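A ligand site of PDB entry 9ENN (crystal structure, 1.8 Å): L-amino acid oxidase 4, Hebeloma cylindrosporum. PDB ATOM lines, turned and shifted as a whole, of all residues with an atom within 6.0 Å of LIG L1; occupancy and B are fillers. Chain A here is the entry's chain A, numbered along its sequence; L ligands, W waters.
The side-chain hydroxyl (OH) of Tyr 404 is in hydrogen-bond range of an oxygen (O3) of LIG L1 (2.7 Å).
O of Ala 505 is in hydrogen-bond range of N2 of LIG L1 (2.8 Å).
The guanidinium group (NE) of Arg 70 is in salt-bridge range of an oxygen (O2) of LIG L1, 2.9 Å away.
OE2 of Glu 235 is in hydrogen-bond range of N1 of LIG L1 (3.3 Å).
O of Ala 505 lies close to N6 of LG2 L2 (3.5 Å).
An oxygen (O8) of LG2 L2 lies within hydrogen-bond range of the backbone NH of Arg 70, at 3.0 Å.
The backbone carbonyl oxygen of Arg 70 sits at hydrogen-bond distance from a nitrogen (N7) of LG2 L2, at 2.8 Å.
An oxygen (O10) of LG2 L2 sits at hydrogen-bond distance from the backbone carbonyl oxygen of Trp 506 (3.1 Å).
The backbone NH of Met 69 lies within hydrogen-bond range of an oxygen (O8) of LG2 L2, 3.1 Å away.
NE1 of Trp 406 sits at hydrogen-bond distance from OH of Tyr 404 (3.0 Å).
The side-chain carboxylate (OE1) of Glu 235 sits at hydrogen-bond distance from the indole nitrogen (NE1) of Trp 506 (2.7 Å).
The side-chain carboxylate of Glu 235 sits close to the backbone carbonyl oxygen of His 504 (2.7 Å).
Trp 224 touches LIG L1 (CZ3 to O1, 3.7 Å).
Phe 239 touches LIG L1.
Trp 406 touches LIG L1 (CZ2 to O3, 3.6 Å).
Phe 469 touches LIG L1.
O of Ala 470 touches C2 of LIG L1, 3.4 Å away.
CD2 of Phe 471 touches O1 of LIG L1, 3.2 Å away.
Trp 506 touches LIG L1 (CZ3 to N2, 3.4 Å).
Hydrophobic or aromatic side chains within 4 Å of LIG L1: Trp 224, Phe 239, Tyr 404, Trp 406, Phe 469, Phe 471, Ala 505 and Trp 506.
Of the 16 residues printed, 11 come within 4 Å of LIG L1.
Water W2 lies within hydrogen-bond range of N8 of LG2 L2 (3.0 Å), O3 of LIG L1 (3.3 Å) and SD of Met 69 (3.6 Å).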
ATOM      1  N   MET A  69      24.159 -27.002   9.978  1.00  0.00           N
ATOM      2  CA  MET A  69      24.845 -26.882   8.695  1.00  0.00           C
ATOM      3  C   MET A  69      26.160 -27.641   8.587  1.00  0.00           C
ATOM      4  O   MET A  69      26.655 -27.789   7.467  1.00  0.00           O
ATOM      5  CB  MET A  69      25.126 -25.399   8.380  1.00  0.00           C
ATOM      6  CG  MET A  69      26.266 -24.769   9.180  1.00  0.00           C
ATOM      7  SD  MET A  69      26.455 -22.993   8.853  1.00  0.00           S
ATOM      8  CE  MET A  69      27.801 -22.593   9.970  1.00  0.00           C
ATOM      9  N   ARG A  70      26.756 -28.113   9.679  1.00  0.00           N
ATOM     10  CA  ARG A  70      28.083 -28.719   9.612  1.00  0.00           C
ATOM     11  C   ARG A  70      28.205 -29.831  10.634  1.00  0.00           C
ATOM     12  O   ARG A  70      27.684 -29.742  11.743  1.00  0.00           O
ATOM     13  CB  ARG A  70      29.170 -27.655   9.817  1.00  0.00           C
ATOM     14  CG  ARG A  70      29.071 -26.898  11.135  1.00  0.00           C
ATOM     15  CD  ARG A  70      30.004 -25.701  11.162  1.00  0.00           C
ATOM     16  NE  ARG A  70      29.831 -24.904  12.366  1.00  0.00           N
ATOM     17  CZ  ARG A  70      30.362 -23.694  12.551  1.00  0.00           C
ATOM     18  NH1 ARG A  70      31.075 -23.104  11.612  1.00  0.00           N
ATOM     19  NH2 ARG A  70      30.171 -23.077  13.709  1.00  0.00           N
ATOM     20  N   TRP A 224      29.489 -15.677  26.329  1.00  0.00           N
ATOM     21  CA  TRP A 224      29.641 -17.120  26.421  1.00  0.00           C
ATOM     22  C   TRP A 224      30.171 -17.550  27.782  1.00  0.00           C
ATOM     23  O   TRP A 224      29.713 -18.543  28.354  1.00  0.00           O
ATOM     24  CB  TRP A 224      30.598 -17.605  25.328  1.00  0.00           C
ATOM     25  CG  TRP A 224      30.840 -19.078  25.343  1.00  0.00           C
ATOM     26  CD1 TRP A 224      31.527 -19.796  26.284  1.00  0.00           C
ATOM     27  CD2 TRP A 224      30.408 -20.023  24.355  1.00  0.00           C
ATOM     28  NE1 TRP A 224      31.551 -21.126  25.947  1.00  0.00           N
ATOM     29  CE2 TRP A 224      30.859 -21.292  24.765  1.00  0.00           C
ATOM     30  CE3 TRP A 224      29.679 -19.919  23.173  1.00  0.00           C
ATOM     31  CZ2 TRP A 224      30.606 -22.445  24.030  1.00  0.00           C
ATOM     32  CZ3 TRP A 224      29.436 -21.061  22.447  1.00  0.00           C
ATOM     33  CH2 TRP A 224      29.889 -22.304  22.878  1.00  0.00           C
ATOM     34  N   GLU A 231      29.646 -26.489  29.657  1.00  0.00           N
ATOM     35  CA  GLU A 231      29.308 -26.318  28.244  1.00  0.00           C
ATOM     36  C   GLU A 231      30.549 -25.941  27.424  1.00  0.00           C
ATOM     37  O   GLU A 231      30.719 -26.421  26.304  1.00  0.00           O
ATOM     38  CB  GLU A 231      28.206 -25.273  28.078  1.00  0.00           C
ATOM     39  CG  GLU A 231      26.820 -25.675  28.576  1.00  0.00           C
ATOM     40  CD  GLU A 231      26.059 -26.617  27.649  1.00  0.00           C
ATOM     41  OE1 GLU A 231      26.688 -27.483  26.996  1.00  0.00           O
ATOM     42  OE2 GLU A 231      24.821 -26.466  27.550  1.00  0.00           O
ATOM     43  N   GLU A 235      31.561 -28.344  24.421  1.00  0.00           N
ATOM     44  CA  GLU A 235      31.605 -27.882  23.041  1.00  0.00           C
ATOM     45  C   GLU A 235      33.012 -28.015  22.467  1.00  0.00           C
ATOM     46  O   GLU A 235      33.140 -28.283  21.262  1.00  0.00           O
ATOM     47  CB  GLU A 235      31.036 -26.473  22.950  1.00  0.00           C
ATOM     48  CG  GLU A 235      29.535 -26.369  23.363  1.00  0.00           C
ATOM     49  CD  GLU A 235      28.589 -27.291  22.568  1.00  0.00           C
ATOM     50  OE1 GLU A 235      28.964 -27.785  21.494  1.00  0.00           O
ATOM     51  OE2 GLU A 235      27.440 -27.511  23.025  1.00  0.00           O
ATOM     52  N   PHE A 239      33.512 -29.836  18.943  1.00  0.00           N
ATOM     53  CA  PHE A 239      34.181 -29.208  17.807  1.00  0.00           C
ATOM     54  C   PHE A 239      35.494 -29.923  17.452  1.00  0.00           C
ATOM     55  O   PHE A 239      36.177 -29.488  16.516  1.00  0.00           O
ATOM     56  CB  PHE A 239      34.463 -27.714  18.064  1.00  0.00           C
ATOM     57  CG  PHE A 239      33.322 -26.795  17.668  1.00  0.00           C
ATOM     58  CD1 PHE A 239      33.111 -26.459  16.337  1.00  0.00           C
ATOM     59  CD2 PHE A 239      32.489 -26.251  18.629  1.00  0.00           C
ATOM     60  CE1 PHE A 239      32.073 -25.611  15.976  1.00  0.00           C
ATOM     61  CE2 PHE A 239      31.452 -25.403  18.269  1.00  0.00           C
ATOM     62  CZ  PHE A 239      31.244 -25.083  16.942  1.00  0.00           C
ATOM     63  N   TRP A 249      35.075 -32.814   8.662  1.00  0.00           N
ATOM     64  CA  TRP A 249      33.953 -31.880   8.587  1.00  0.00           C
ATOM     65  C   TRP A 249      33.169 -32.136   7.304  1.00  0.00           C
ATOM     66  O   TRP A 249      33.734 -32.097   6.200  1.00  0.00           O
ATOM     67  CB  TRP A 249      34.457 -30.452   8.621  1.00  0.00           C
ATOM     68  CG  TRP A 249      34.863 -29.934   9.973  1.00  0.00           C
ATOM     69  CD1 TRP A 249      36.128 -29.825  10.455  1.00  0.00           C
ATOM     70  CD2 TRP A 249      33.999 -29.453  11.010  1.00  0.00           C
ATOM     71  NE1 TRP A 249      36.106 -29.304  11.720  1.00  0.00           N
ATOM     72  CE2 TRP A 249      34.814 -29.071  12.086  1.00  0.00           C
ATOM     73  CE3 TRP A 249      32.611 -29.315  11.125  1.00  0.00           C
ATOM     74  CZ2 TRP A 249      34.287 -28.553  13.276  1.00  0.00           C
ATOM     75  CZ3 TRP A 249      32.095 -28.790  12.294  1.00  0.00           C
ATOM     76  CH2 TRP A 249      32.927 -28.423  13.349  1.00  0.00           C
ATOM     77  N   TYR A 404      26.353 -14.833  11.574  1.00  0.00           N
ATOM     78  CA  TYR A 404      25.942 -15.964  12.417  1.00  0.00           C
ATOM     79  C   TYR A 404      26.433 -15.626  13.825  1.00  0.00           C
ATOM     80  O   TYR A 404      27.640 -15.541  14.059  1.00  0.00           O
ATOM     81  CB  TYR A 404      26.519 -17.277  11.894  1.00  0.00           C
ATOM     82  CG  TYR A 404      26.250 -18.505  12.744  1.00  0.00           C
ATOM     83  CD1 TYR A 404      25.142 -18.585  13.587  1.00  0.00           C
ATOM     84  CD2 TYR A 404      27.135 -19.577  12.720  1.00  0.00           C
ATOM     85  CE1 TYR A 404      24.919 -19.712  14.373  1.00  0.00           C
ATOM     86  CE2 TYR A 404      26.920 -20.698  13.502  1.00  0.00           C
ATOM     87  CZ  TYR A 404      25.812 -20.761  14.323  1.00  0.00           C
ATOM     88  OH  TYR A 404      25.612 -21.884  15.104  1.00  0.00           O
ATOM     89  N   TRP A 406      25.839 -15.746  18.324  1.00  0.00           N
ATOM     90  CA  TRP A 406      25.423 -16.392  19.559  1.00  0.00           C
ATOM     91  C   TRP A 406      25.251 -15.388  20.693  1.00  0.00           C
ATOM     92  O   TRP A 406      25.620 -14.217  20.581  1.00  0.00           O
ATOM     93  CB  TRP A 406      26.459 -17.447  19.988  1.00  0.00           C
ATOM     94  CG  TRP A 406      26.667 -18.581  19.040  1.00  0.00           C
ATOM     95  CD1 TRP A 406      25.751 -19.120  18.182  1.00  0.00           C
ATOM     96  CD2 TRP A 406      27.878 -19.336  18.860  1.00  0.00           C
ATOM     97  NE1 TRP A 406      26.316 -20.163  17.485  1.00  0.00           N
ATOM     98  CE2 TRP A 406      27.617 -20.328  17.883  1.00  0.00           C
ATOM     99  CE3 TRP A 406      29.151 -19.279  19.428  1.00  0.00           C
ATOM    100  CZ2 TRP A 406      28.585 -21.237  17.466  1.00  0.00           C
ATOM    101  CZ3 TRP A 406      30.113 -20.203  19.026  1.00  0.00           C
ATOM    102  CH2 TRP A 406      29.822 -21.165  18.044  1.00  0.00           C
ATOM    103  N   PHE A 469      18.780 -23.340  21.229  1.00  0.00           N
ATOM    104  CA  PHE A 469      19.165 -24.644  21.728  1.00  0.00           C
ATOM    105  C   PHE A 469      19.505 -24.516  23.199  1.00  0.00           C
ATOM    106  O   PHE A 469      19.672 -23.410  23.731  1.00  0.00           O
ATOM    107  CB  PHE A 469      20.367 -25.249  20.941  1.00  0.00           C
ATOM    108  CG  PHE A 469      21.346 -24.226  20.439  1.00  0.00           C
ATOM    109  CD1 PHE A 469      22.028 -23.414  21.323  1.00  0.00           C
ATOM    110  CD2 PHE A 469      21.597 -24.089  19.082  1.00  0.00           C
ATOM    111  CE1 PHE A 469      22.930 -22.454  20.868  1.00  0.00           C
ATOM    112  CE2 PHE A 469      22.499 -23.141  18.608  1.00  0.00           C
ATOM    113  CZ  PHE A 469      23.164 -22.313  19.514  1.00  0.00           C
ATOM    114  N   ALA A 470      19.574 -25.665  23.855  1.00  0.00           N
ATOM    115  CA  ALA A 470      20.058 -25.700  25.225  1.00  0.00           C
ATOM    116  C   ALA A 470      21.460 -25.107  25.291  1.00  0.00           C
ATOM    117  O   ALA A 470      22.297 -25.375  24.434  1.00  0.00           O
ATOM    118  CB  ALA A 470      20.045 -27.140  25.744  1.00  0.00           C
ATOM    119  N   PHE A 471      21.697 -24.269  26.307  1.00  0.00           N
ATOM    120  CA  PHE A 471      23.019 -23.698  26.590  1.00  0.00           C
ATOM    121  C   PHE A 471      23.021 -23.445  28.103  1.00  0.00           C
ATOM    122  O   PHE A 471      22.694 -22.352  28.561  1.00  0.00           O
ATOM    123  CB  PHE A 471      23.292 -22.427  25.794  1.00  0.00           C
ATOM    124  CG  PHE A 471      24.736 -21.974  25.802  1.00  0.00           C
ATOM    125  CD1 PHE A 471      25.665 -22.530  26.677  1.00  0.00           C
ATOM    126  CD2 PHE A 471      25.175 -20.984  24.928  1.00  0.00           C
ATOM    127  CE1 PHE A 471      26.991 -22.100  26.674  1.00  0.00           C
ATOM    128  CE2 PHE A 471      26.490 -20.565  24.915  1.00  0.00           C
ATOM    129  CZ  PHE A 471      27.410 -21.120  25.800  1.00  0.00           C
ATOM    130  N   PHE A 472      23.351 -24.490  28.864  1.00  0.00           N
ATOM    131  CA  PHE A 472      23.105 -24.508  30.299  1.00  0.00           C
ATOM    132  C   PHE A 472      23.957 -23.496  31.058  1.00  0.00           C
ATOM    133  O   PHE A 472      25.131 -23.280  30.743  1.00  0.00           O
ATOM    134  CB  PHE A 472      23.386 -25.910  30.872  1.00  0.00           C
ATOM    135  CG  PHE A 472      22.321 -26.941  30.604  1.00  0.00           C
ATOM    136  CD1 PHE A 472      21.201 -26.673  29.829  1.00  0.00           C
ATOM    137  CD2 PHE A 472      22.450 -28.218  31.148  1.00  0.00           C
ATOM    138  CE1 PHE A 472      20.229 -27.650  29.606  1.00  0.00           C
ATOM    139  CE2 PHE A 472      21.499 -29.206  30.916  1.00  0.00           C
ATOM    140  CZ  PHE A 472      20.381 -28.912  30.162  1.00  0.00           C
ATOM    141  N   HIS A 504      24.635 -30.458  23.444  1.00  0.00           N
ATOM    142  CA  HIS A 504      23.724 -29.368  23.136  1.00  0.00           C
ATOM    143  C   HIS A 504      24.133 -28.663  21.858  1.00  0.00           C
ATOM    144  O   HIS A 504      25.317 -28.416  21.614  1.00  0.00           O
ATOM    145  CB  HIS A 504      23.702 -28.378  24.297  1.00  0.00           C
ATOM    146  CG  HIS A 504      23.058 -28.915  25.525  1.00  0.00           C
ATOM    147  ND1 HIS A 504      23.316 -28.419  26.793  1.00  0.00           N
ATOM    148  CD2 HIS A 504      22.163 -29.909  25.699  1.00  0.00           C
ATOM    149  CE1 HIS A 504      22.603 -29.088  27.677  1.00  0.00           C
ATOM    150  NE2 HIS A 504      21.888 -30.001  27.037  1.00  0.00           N
ATOM    151  N   ALA A 505      23.122 -28.304  21.058  1.00  0.00           N
ATOM    152  CA  ALA A 505      23.293 -27.567  19.811  1.00  0.00           C
ATOM    153  C   ALA A 505      23.963 -28.402  18.731  1.00  0.00           C
ATOM    154  O   ALA A 505      24.593 -27.864  17.821  1.00  0.00           O
ATOM    155  CB  ALA A 505      24.067 -26.261  20.033  1.00  0.00           C
ATOM    156  N   TRP A 506      23.818 -29.731  18.837  1.00  0.00           N
ATOM    157  CA  TRP A 506      24.252 -30.652  17.801  1.00  0.00           C
ATOM    158  C   TRP A 506      23.160 -31.673  17.504  1.00  0.00           C
ATOM    159  O   TRP A 506      22.384 -32.059  18.389  1.00  0.00           O
ATOM    160  CB  TRP A 506      25.509 -31.407  18.204  1.00  0.00           C
ATOM    161  CG  TRP A 506      26.666 -30.535  18.418  1.00  0.00           C
ATOM    162  CD1 TRP A 506      27.128 -30.072  19.617  1.00  0.00           C
ATOM    163  CD2 TRP A 506      27.519 -29.973  17.414  1.00  0.00           C
ATOM    164  NE1 TRP A 506      28.221 -29.265  19.424  1.00  0.00           N
ATOM    165  CE2 TRP A 506      28.490 -29.191  18.071  1.00  0.00           C
ATOM    166  CE3 TRP A 506      27.566 -30.065  16.023  1.00  0.00           C
ATOM    167  CZ2 TRP A 506      29.496 -28.505  17.387  1.00  0.00           C
ATOM    168  CZ3 TRP A 506      28.569 -29.393  15.338  1.00  0.00           C
ATOM    169  CH2 TRP A 506      29.519 -28.617  16.025  1.00  0.00           C
HETATM  170  O1  LIG L   1      26.158 -22.707  22.417  1.00  0.00           O
HETATM  171  C1  LIG L   1      26.183 -23.940  22.459  1.00  0.00           C
HETATM  172  C2  LIG L   1      25.518 -24.817  23.548  1.00  0.00           C
HETATM  173  N1  LIG L   1      26.835 -24.630  21.514  1.00  0.00           N
HETATM  174  C3  LIG L   1      27.526 -24.042  20.373  1.00  0.00           C
HETATM  175  C4  LIG L   1      28.266 -25.106  19.609  1.00  0.00           C
HETATM  176  C5  LIG L   1      28.180 -25.005  18.099  1.00  0.00           C
HETATM  177  C6  LIG L   1      26.808 -24.683  17.527  1.00  0.00           C
HETATM  178  C7  LIG L   1      26.549 -25.336  16.178  1.00  0.00           C
HETATM  179  N2  LIG L   1      26.611 -26.789  16.279  1.00  0.00           N
HETATM  180  C8  LIG L   1      27.599 -24.910  15.158  1.00  0.00           C
HETATM  181  O2  LIG L   1      28.307 -25.759  14.621  1.00  0.00           O
HETATM  182  O3  LIG L   1      27.647 -23.689  14.936  1.00  0.00           O
HETATM  183  P1  LG2 L   2      13.662 -29.684  16.923  1.00  0.00           P
HETATM  184  O1  LG2 L   2      13.381 -28.346  17.534  1.00  0.00           O
HETATM  185  O2  LG2 L   2      14.455 -29.758  15.659  1.00  0.00           O
HETATM  186  O3  LG2 L   2      12.279 -30.446  16.685  1.00  0.00           O
HETATM  187  C1  LG2 L   2      11.133 -30.223  17.554  1.00  0.00           C
HETATM  188  C2  LG2 L   2       9.876 -30.303  16.714  1.00  0.00           C
HETATM  189  O4  LG2 L   2       8.711 -30.054  17.540  1.00  0.00           O
HETATM  190  C3  LG2 L   2       9.778 -29.300  15.550  1.00  0.00           C
HETATM  191  O5  LG2 L   2       9.427 -29.937  14.331  1.00  0.00           O
HETATM  192  C4  LG2 L   2       8.686 -28.318  16.005  1.00  0.00           C
HETATM  193  O6  LG2 L   2       7.950 -27.762  14.943  1.00  0.00           O
HETATM  194  C5  LG2 L   2       7.789 -29.227  16.847  1.00  0.00           C
HETATM  195  N1  LG2 L   2       6.970 -28.581  17.845  1.00  0.00           N
HETATM  196  C6  LG2 L   2       7.269 -27.469  18.593  1.00  0.00           C
HETATM  197  N2  LG2 L   2       6.309 -27.158  19.436  1.00  0.00           N
HETATM  198  C7  LG2 L   2       5.330 -28.130  19.236  1.00  0.00           C
HETATM  199  C8  LG2 L   2       4.080 -28.355  19.824  1.00  0.00           C
HETATM  200  N3  LG2 L   2       3.563 -27.603  20.794  1.00  0.00           N
HETATM  201  N4  LG2 L   2       3.358 -29.421  19.388  1.00  0.00           N
HETATM  202  C9  LG2 L   2       3.886 -30.183  18.418  1.00  0.00           C
HETATM  203  N5  LG2 L   2       5.049 -30.065  17.788  1.00  0.00           N
HETATM  204  C10 LG2 L   2       5.737 -29.010  18.251  1.00  0.00           C
HETATM  205  N6  LG2 L   2      23.614 -29.274  14.823  1.00  0.00           N
HETATM  206  C11 LG2 L   2      24.587 -29.914  14.105  1.00  0.00           C
HETATM  207  O7  LG2 L   2      24.731 -31.119  14.189  1.00  0.00           O
HETATM  208  N7  LG2 L   2      25.401 -29.126  13.310  1.00  0.00           N
HETATM  209  C12 LG2 L   2      25.291 -27.755  13.196  1.00  0.00           C
HETATM  210  O8  LG2 L   2      26.052 -27.152  12.442  1.00  0.00           O
HETATM  211  C13 LG2 L   2      24.307 -27.121  13.964  1.00  0.00           C
HETATM  212  N8  LG2 L   2      24.157 -25.756  13.954  1.00  0.00           N
HETATM  213  C14 LG2 L   2      23.028 -25.164  14.476  1.00  0.00           C
HETATM  214  C15 LG2 L   2      22.771 -23.816  14.279  1.00  0.00           C
HETATM  215  C16 LG2 L   2      21.612 -23.244  14.738  1.00  0.00           C
HETATM  216  C17 LG2 L   2      21.354 -21.779  14.499  1.00  0.00           C
HETATM  217  C18 LG2 L   2      20.665 -24.062  15.435  1.00  0.00           C
HETATM  218  C19 LG2 L   2      19.376 -23.472  15.961  1.00  0.00           C
HETATM  219  C20 LG2 L   2      20.921 -25.390  15.640  1.00  0.00           C
HETATM  220  C21 LG2 L   2      22.104 -25.958  15.174  1.00  0.00           C
HETATM  221  N9  LG2 L   2      22.438 -27.319  15.436  1.00  0.00           N
HETATM  222  C22 LG2 L   2      23.456 -27.916  14.762  1.00  0.00           C
HETATM  223  C23 LG2 L   2      21.654 -28.098  16.429  1.00  0.00           C
HETATM  224  C24 LG2 L   2      20.568 -28.959  15.780  1.00  0.00           C
HETATM  225  O9  LG2 L   2      19.916 -28.224  14.771  1.00  0.00           O
HETATM  226  C25 LG2 L   2      19.575 -29.357  16.869  1.00  0.00           C
HETATM  227  O10 LG2 L   2      20.274 -29.790  18.048  1.00  0.00           O
HETATM  228  C26 LG2 L   2      18.585 -30.450  16.469  1.00  0.00           C
HETATM  229  O11 LG2 L   2      18.113 -30.233  15.137  1.00  0.00           O
HETATM  230  C27 LG2 L   2      17.399 -30.476  17.401  1.00  0.00           C
HETATM  231  O12 LG2 L   2      16.487 -31.561  17.074  1.00  0.00           O
HETATM  232  P2  LG2 L   2      15.276 -31.903  18.058  1.00  0.00           P
HETATM  233  O13 LG2 L   2      14.516 -33.001  17.396  1.00  0.00           O
HETATM  234  O14 LG2 L   2      15.775 -32.062  19.456  1.00  0.00           O
HETATM  235  O15 LG2 L   2      14.403 -30.556  18.040  1.00  0.00           O
HETATM  236  O   HOH W   1      25.811 -20.509  21.496  1.00  0.00           O
HETATM  237  O   HOH W   2      25.943 -24.123  12.185  1.00  0.00           O
